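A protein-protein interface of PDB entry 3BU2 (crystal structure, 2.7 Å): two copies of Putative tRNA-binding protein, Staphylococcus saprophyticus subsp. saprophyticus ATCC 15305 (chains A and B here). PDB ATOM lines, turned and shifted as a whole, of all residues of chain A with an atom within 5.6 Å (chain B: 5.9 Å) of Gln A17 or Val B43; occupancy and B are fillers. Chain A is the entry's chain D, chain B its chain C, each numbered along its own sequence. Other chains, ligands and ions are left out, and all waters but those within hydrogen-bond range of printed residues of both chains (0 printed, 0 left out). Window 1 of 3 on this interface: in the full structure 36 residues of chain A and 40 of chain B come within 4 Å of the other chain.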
ATOM      1  N   MET A   1     -31.833   7.564 -22.822  1.00  0.00           N
ATOM      2  CA  MET A   1     -31.181   6.379 -23.455  1.00  0.00           C
ATOM      3  C   MET A   1     -32.217   5.470 -24.083  1.00  0.00           C
ATOM      4  O   MET A   1     -33.410   5.577 -23.790  1.00  0.00           O
ATOM      5  CB  MET A   1     -30.368   5.584 -22.427  1.00  0.00           C
ATOM      6  CG  MET A   1     -31.194   4.889 -21.356  1.00  0.00           C
ATOM      7  SD  MET A   1     -30.083   3.920 -20.084  1.00  0.00           S
ATOM      8  CE  MET A   1     -30.134   2.170 -20.917  1.00  0.00           C
ATOM      9  N   ASN A   2     -31.746   4.564 -24.936  1.00  0.00           N
ATOM     10  CA  ASN A   2     -32.618   3.632 -25.637  1.00  0.00           C
ATOM     11  C   ASN A   2     -32.051   2.207 -25.660  1.00  0.00           C
ATOM     12  O   ASN A   2     -30.848   2.010 -25.504  1.00  0.00           O
ATOM     13  CB  ASN A   2     -32.840   4.163 -27.047  1.00  0.00           C
ATOM     14  CG  ASN A   2     -33.112   5.663 -27.056  1.00  0.00           C
ATOM     15  OD1 ASN A   2     -34.187   6.115 -26.647  1.00  0.00           O
ATOM     16  ND2 ASN A   2     -32.127   6.444 -27.505  1.00  0.00           N
ATOM     17  N   LEU A   3     -32.927   1.224 -25.855  1.00  0.00           N
ATOM     18  CA  LEU A   3     -32.539  -0.188 -25.870  1.00  0.00           C
ATOM     19  C   LEU A   3     -33.000  -0.984 -27.096  1.00  0.00           C
ATOM     20  O   LEU A   3     -34.202  -1.083 -27.350  1.00  0.00           O
ATOM     21  CB  LEU A   3     -33.085  -0.881 -24.619  1.00  0.00           C
ATOM     22  CG  LEU A   3     -32.980  -2.404 -24.586  1.00  0.00           C
ATOM     23  CD1 LEU A   3     -31.521  -2.808 -24.560  1.00  0.00           C
ATOM     24  CD2 LEU A   3     -33.697  -2.944 -23.364  1.00  0.00           C
ATOM     25  N   PHE A  15     -28.513  -3.914 -26.858  1.00  0.00           N
ATOM     26  CA  PHE A  15     -27.833  -2.695 -27.263  1.00  0.00           C
ATOM     27  C   PHE A  15     -28.291  -1.469 -26.480  1.00  0.00           C
ATOM     28  O   PHE A  15     -29.427  -1.007 -26.641  1.00  0.00           O
ATOM     29  CB  PHE A  15     -28.071  -2.440 -28.745  1.00  0.00           C
ATOM     30  CG  PHE A  15     -27.296  -3.344 -29.649  1.00  0.00           C
ATOM     31  CD1 PHE A  15     -25.923  -3.193 -29.787  1.00  0.00           C
ATOM     32  CD2 PHE A  15     -27.942  -4.333 -30.385  1.00  0.00           C
ATOM     33  CE1 PHE A  15     -25.206  -4.013 -30.649  1.00  0.00           C
ATOM     34  CE2 PHE A  15     -27.235  -5.159 -31.250  1.00  0.00           C
ATOM     35  CZ  PHE A  15     -25.865  -5.000 -31.384  1.00  0.00           C
ATOM     36  N   LEU A  16     -27.411  -0.941 -25.636  1.00  0.00           N
ATOM     37  CA  LEU A  16     -27.737   0.252 -24.867  1.00  0.00           C
ATOM     38  C   LEU A  16     -27.046   1.437 -25.508  1.00  0.00           C
ATOM     39  O   LEU A  16     -25.818   1.436 -25.655  1.00  0.00           O
ATOM     40  CB  LEU A  16     -27.254   0.138 -23.419  1.00  0.00           C
ATOM     41  CG  LEU A  16     -28.136  -0.528 -22.361  1.00  0.00           C
ATOM     42  CD1 LEU A  16     -28.350  -1.991 -22.684  1.00  0.00           C
ATOM     43  CD2 LEU A  16     -27.459  -0.390 -21.009  1.00  0.00           C
ATOM     44  N   GLN A  17     -27.830   2.433 -25.909  1.00  0.00           N
ATOM     45  CA  GLN A  17     -27.276   3.646 -26.498  1.00  0.00           C
ATOM     46  C   GLN A  17     -27.486   4.718 -25.428  1.00  0.00           C
ATOM     47  O   GLN A  17     -28.523   4.747 -24.768  1.00  0.00           O
ATOM     48  CB  GLN A  17     -28.018   4.014 -27.783  1.00  0.00           C
ATOM     49  CG  GLN A  17     -28.169   2.861 -28.765  1.00  0.00           C
ATOM     50  CD  GLN A  17     -26.949   2.646 -29.641  1.00  0.00           C
ATOM     51  OE1 GLN A  17     -26.885   3.130 -30.779  1.00  0.00           O
ATOM     52  NE2 GLN A  17     -25.969   1.918 -29.115  1.00  0.00           N
ATOM     53  N   ILE A  18     -26.495   5.583 -25.241  1.00  0.00           N
ATOM     54  CA  ILE A  18     -26.582   6.623 -24.219  1.00  0.00           C
ATOM     55  C   ILE A  18     -26.128   7.974 -24.742  1.00  0.00           C
ATOM     56  O   ILE A  18     -25.166   8.060 -25.499  1.00  0.00           O
ATOM     57  CB  ILE A  18     -25.711   6.250 -22.991  1.00  0.00           C
ATOM     58  CG1 ILE A  18     -26.233   4.950 -22.364  1.00  0.00           C
ATOM     59  CG2 ILE A  18     -25.705   7.390 -21.975  1.00  0.00           C
ATOM     60  CD1 ILE A  18     -25.368   4.408 -21.231  1.00  0.00           C
ATOM     61  N   ASN A  19     -26.841   9.023 -24.346  1.00  0.00           N
ATOM     62  CA  ASN A  19     -26.497  10.382 -24.745  1.00  0.00           C
ATOM     63  C   ASN A  19     -25.764  11.028 -23.580  1.00  0.00           C
ATOM     64  O   ASN A  19     -26.334  11.220 -22.503  1.00  0.00           O
ATOM     65  CB  ASN A  19     -27.750  11.202 -25.058  1.00  0.00           C
ATOM     66  CG  ASN A  19     -28.486  10.703 -26.279  1.00  0.00           C
ATOM     67  OD1 ASN A  19     -29.681  10.397 -26.219  1.00  0.00           O
ATOM     68  ND2 ASN A  19     -27.781  10.621 -27.400  1.00  0.00           N
ATOM     69  N   PRO A  20     -24.481  11.358 -23.764  1.00  0.00           N
ATOM     70  CA  PRO A  20     -23.789  11.983 -22.635  1.00  0.00           C
ATOM     71  C   PRO A  20     -24.586  13.218 -22.230  1.00  0.00           C
ATOM     72  O   PRO A  20     -25.543  13.597 -22.902  1.00  0.00           O
ATOM     73  CB  PRO A  20     -22.422  12.338 -23.218  1.00  0.00           C
ATOM     74  CG  PRO A  20     -22.214  11.282 -24.265  1.00  0.00           C
ATOM     75  CD  PRO A  20     -23.583  11.201 -24.921  1.00  0.00           C
ATOM     76  N   MET A 150     -32.747   3.391 -32.692  1.00  0.00           N
ATOM     77  CA  MET A 150     -31.295   3.277 -32.815  1.00  0.00           C
ATOM     78  C   MET A 150     -30.711   3.760 -34.143  1.00  0.00           C
ATOM     79  O   MET A 150     -31.332   3.630 -35.195  1.00  0.00           O
ATOM     80  CB  MET A 150     -30.859   1.828 -32.583  1.00  0.00           C
ATOM     81  CG  MET A 150     -29.439   1.543 -33.027  1.00  0.00           C
ATOM     82  SD  MET A 150     -28.870  -0.265 -32.620  1.00  0.00           S
ATOM     83  CE  MET A 150     -27.208   0.171 -31.718  1.00  0.00           C
ATOM     84  N   VAL A 151     -29.506   4.316 -34.068  1.00  0.00           N
ATOM     85  CA  VAL A 151     -28.798   4.819 -35.234  1.00  0.00           C
ATOM     86  C   VAL A 151     -27.572   3.938 -35.454  1.00  0.00           C
ATOM     87  O   VAL A 151     -26.686   3.878 -34.602  1.00  0.00           O
ATOM     88  CB  VAL A 151     -28.332   6.280 -35.018  1.00  0.00           C
ATOM     89  CG1 VAL A 151     -27.628   6.794 -36.266  1.00  0.00           C
ATOM     90  CG2 VAL A 151     -29.522   7.160 -34.685  1.00  0.00           C
ATOM     91  N   TYR B  25     -14.913   5.717 -31.541  1.00  0.00           N
ATOM     92  CA  TYR B  25     -15.528   5.059 -30.409  1.00  0.00           C
ATOM     93  C   TYR B  25     -14.497   4.088 -29.845  1.00  0.00           C
ATOM     94  O   TYR B  25     -13.725   3.484 -30.595  1.00  0.00           O
ATOM     95  CB  TYR B  25     -16.766   4.289 -30.862  1.00  0.00           C
ATOM     96  CG  TYR B  25     -18.037   5.107 -30.904  1.00  0.00           C
ATOM     97  CD1 TYR B  25     -19.191   4.597 -31.488  1.00  0.00           C
ATOM     98  CD2 TYR B  25     -18.102   6.367 -30.308  1.00  0.00           C
ATOM     99  CE1 TYR B  25     -20.383   5.318 -31.473  1.00  0.00           C
ATOM    100  CE2 TYR B  25     -19.284   7.094 -30.287  1.00  0.00           C
ATOM    101  CZ  TYR B  25     -20.425   6.566 -30.870  1.00  0.00           C
ATOM    102  OH  TYR B  25     -21.608   7.279 -30.834  1.00  0.00           O
ATOM    103  N   ILE B  36     -18.837   1.051 -24.184  1.00  0.00           N
ATOM    104  CA  ILE B  36     -18.389   1.831 -25.319  1.00  0.00           C
ATOM    105  C   ILE B  36     -18.443   3.312 -24.956  1.00  0.00           C
ATOM    106  O   ILE B  36     -19.426   3.794 -24.400  1.00  0.00           O
ATOM    107  CB  ILE B  36     -19.236   1.531 -26.596  1.00  0.00           C
ATOM    108  CG1 ILE B  36     -19.177   2.718 -27.545  1.00  0.00           C
ATOM    109  CG2 ILE B  36     -20.665   1.171 -26.231  1.00  0.00           C
ATOM    110  CD1 ILE B  36     -19.936   2.504 -28.820  1.00  0.00           C
ATOM    111  N   GLN B  37     -17.367   4.027 -25.259  1.00  0.00           N
ATOM    112  CA  GLN B  37     -17.287   5.448 -24.951  1.00  0.00           C
ATOM    113  C   GLN B  37     -16.687   6.276 -26.079  1.00  0.00           C
ATOM    114  O   GLN B  37     -15.884   5.791 -26.873  1.00  0.00           O
ATOM    115  CB  GLN B  37     -16.491   5.657 -23.650  1.00  0.00           C
ATOM    116  CG  GLN B  37     -15.332   4.686 -23.450  1.00  0.00           C
ATOM    117  CD  GLN B  37     -14.701   4.775 -22.061  1.00  0.00           C
ATOM    118  OE1 GLN B  37     -14.106   5.789 -21.699  1.00  0.00           O
ATOM    119  NE2 GLN B  37     -14.830   3.705 -21.281  1.00  0.00           N
ATOM    120  N   ASN B  38     -17.120   7.530 -26.152  1.00  0.00           N
ATOM    121  CA  ASN B  38     -16.644   8.480 -27.150  1.00  0.00           C
ATOM    122  C   ASN B  38     -16.002   9.611 -26.360  1.00  0.00           C
ATOM    123  O   ASN B  38     -16.692  10.320 -25.627  1.00  0.00           O
ATOM    124  CB  ASN B  38     -17.814   9.013 -27.965  1.00  0.00           C
ATOM    125  CG  ASN B  38     -17.373   9.957 -29.062  1.00  0.00           C
ATOM    126  OD1 ASN B  38     -16.653   9.562 -29.982  1.00  0.00           O
ATOM    127  ND2 ASN B  38     -17.799  11.214 -28.972  1.00  0.00           N
ATOM    128  N   GLU B  41     -16.528  10.265 -22.158  1.00  0.00           N
ATOM    129  CA  GLU B  41     -17.889   9.920 -21.754  1.00  0.00           C
ATOM    130  C   GLU B  41     -18.322   8.552 -22.275  1.00  0.00           C
ATOM    131  O   GLU B  41     -17.946   8.156 -23.374  1.00  0.00           O
ATOM    132  CB  GLU B  41     -18.883  10.971 -22.271  1.00  0.00           C
ATOM    133  CG  GLU B  41     -18.830  12.332 -21.580  1.00  0.00           C
ATOM    134  CD  GLU B  41     -19.216  12.259 -20.105  1.00  0.00           C
ATOM    135  OE1 GLU B  41     -18.405  11.731 -19.304  1.00  0.00           O
ATOM    136  OE2 GLU B  41     -20.329  12.722 -19.751  1.00  0.00           O
ATOM    137  N   VAL B  42     -19.111   7.832 -21.484  1.00  0.00           N
ATOM    138  CA  VAL B  42     -19.597   6.542 -21.922  1.00  0.00           C
ATOM    139  C   VAL B  42     -20.802   6.872 -22.797  1.00  0.00           C
ATOM    140  O   VAL B  42     -21.629   7.704 -22.429  1.00  0.00           O
ATOM    141  CB  VAL B  42     -20.023   5.640 -20.738  1.00  0.00           C
ATOM    142  CG1 VAL B  42     -19.057   5.813 -19.583  1.00  0.00           C
ATOM    143  CG2 VAL B  42     -21.433   5.942 -20.319  1.00  0.00           C
ATOM    144  N   VAL B  43     -20.890   6.233 -23.959  1.00  0.00           N
ATOM    145  CA  VAL B  43     -21.981   6.502 -24.886  1.00  0.00           C
ATOM    146  C   VAL B  43     -22.838   5.277 -25.160  1.00  0.00           C
ATOM    147  O   VAL B  43     -23.720   5.307 -26.023  1.00  0.00           O
ATOM    148  CB  VAL B  43     -21.441   7.032 -26.222  1.00  0.00           C
ATOM    149  CG1 VAL B  43     -20.698   8.327 -25.995  1.00  0.00           C
ATOM    150  CG2 VAL B  43     -20.521   6.004 -26.855  1.00  0.00           C
ATOM    151  N   GLY B  44     -22.580   4.195 -24.433  1.00  0.00           N
ATOM    152  CA  GLY B  44     -23.370   2.999 -24.635  1.00  0.00           C
ATOM    153  C   GLY B  44     -22.795   1.726 -24.063  1.00  0.00           C
ATOM    154  O   GLY B  44     -21.711   1.724 -23.478  1.00  0.00           O
ATOM    155  N   TYR B  45     -23.538   0.637 -24.244  1.00  0.00           N
ATOM    156  CA  TYR B  45     -23.135  -0.675 -23.767  1.00  0.00           C
ATOM    157  C   TYR B  45     -23.656  -1.760 -24.681  1.00  0.00           C
ATOM    158  O   TYR B  45     -24.726  -1.630 -25.272  1.00  0.00           O
ATOM    159  CB  TYR B  45     -23.699  -0.941 -22.370  1.00  0.00           C
ATOM    160  CG  TYR B  45     -22.972  -0.248 -21.250  1.00  0.00           C
ATOM    161  CD1 TYR B  45     -21.784  -0.764 -20.746  1.00  0.00           C
ATOM    162  CD2 TYR B  45     -23.467   0.935 -20.704  1.00  0.00           C
ATOM    163  CE1 TYR B  45     -21.107  -0.119 -19.722  1.00  0.00           C
ATOM    164  CE2 TYR B  45     -22.798   1.587 -19.687  1.00  0.00           C
ATOM    165  CZ  TYR B  45     -21.622   1.059 -19.201  1.00  0.00           C
ATOM    166  OH  TYR B  45     -20.950   1.713 -18.206  1.00  0.00           O
ATOM    167  N   ASN B  46     -22.888  -2.831 -24.789  1.00  0.00           N
ATOM    168  CA  ASN B  46     -23.275  -3.995 -25.566  1.00  0.00           C
ATOM    169  C   ASN B  46     -23.145  -5.112 -24.553  1.00  0.00           C
ATOM    170  O   ASN B  46     -22.032  -5.541 -24.244  1.00  0.00           O
ATOM    171  CB  ASN B  46     -22.302  -4.257 -26.713  1.00  0.00           C
ATOM    172  CG  ASN B  46     -22.440  -3.261 -27.835  1.00  0.00           C
ATOM    173  OD1 ASN B  46     -21.692  -3.310 -28.799  1.00  0.00           O
ATOM    174  ND2 ASN B  46     -23.394  -2.351 -27.717  1.00  0.00           N
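The backbone NH (N) of Ile A18 sits at hydrogen-bond distance from the backbone carbonyl oxygen (O) of Val B43.
The backbone carbonyl oxygen (O) of Tyr B45 is in hydrogen-bond range of the backbone NH (N) of Leu A16 (2.8 Å).
O of Ile B36 sits at hydrogen-bond distance from N of Val B43, 2.9 Å away.
N of Ile B36 lies close to O of Gly B44, at 3.0 Å.
The backbone NH (N) of Gln A17 is in hydrogen-bond range of the backbone carbonyl oxygen (O) of Asn A2 (3.1 Å).
Among the printed residues, pairs that only touch across the chains: Leu A16 with Gly B44, Phe A15 with Asn B46, Pro A20 with Val B43, Phe A15 with Tyr B45, Gln A17 with Val B43, Pro A20 with Glu B41 and Ile A18 with Tyr B45.
Printed residues of chain B within 4 Å of Gln A17: Val B43.
Of chain A, only Gln A17 (3.9 Å), Ile A18 (2.9 Å) and Pro A20 (3.7 Å) come within 4 Å of Val B43.
Printed residues of chain B within 4 Å of Pro A20: Glu B41 (3.9 Å) and Val B43 (3.7 Å).
Printed residues of chain B within 4 Å of Ile A18: Val B43 and Tyr B45.
Printed residues of chain A within 4 Å of Asn B46: Phe A15.
The nearest residue of chain A that does not touch Val B43 is Leu A16 (4.4 Å).
The nearest printed residue of chain B that does not touch Pro A20 is Val B42 (4.1 Å).
Hydrophobic or aromatic side chains of chain B within 4 Å of the printed part of chain A: Val B43 and Tyr B45.
Of the 11 printed residues of chain A, 5 touch a printed residue of chain B.
Printed residues of chain A that touch a printed residue of chain B: Phe A15, Leu A16, Gln A17, Ile A18 and Pro A20.
Hydrophobic or aromatic side chains of chain A that line the printed part of chain B: Phe A15, Leu A16, Ile A18 and Pro A20.
Among the printed residues, no Asp or Glu carboxylate lies within 4 Å of a Lys or Arg side-chain nitrogen of the other chain.
No position is printed for both chains.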
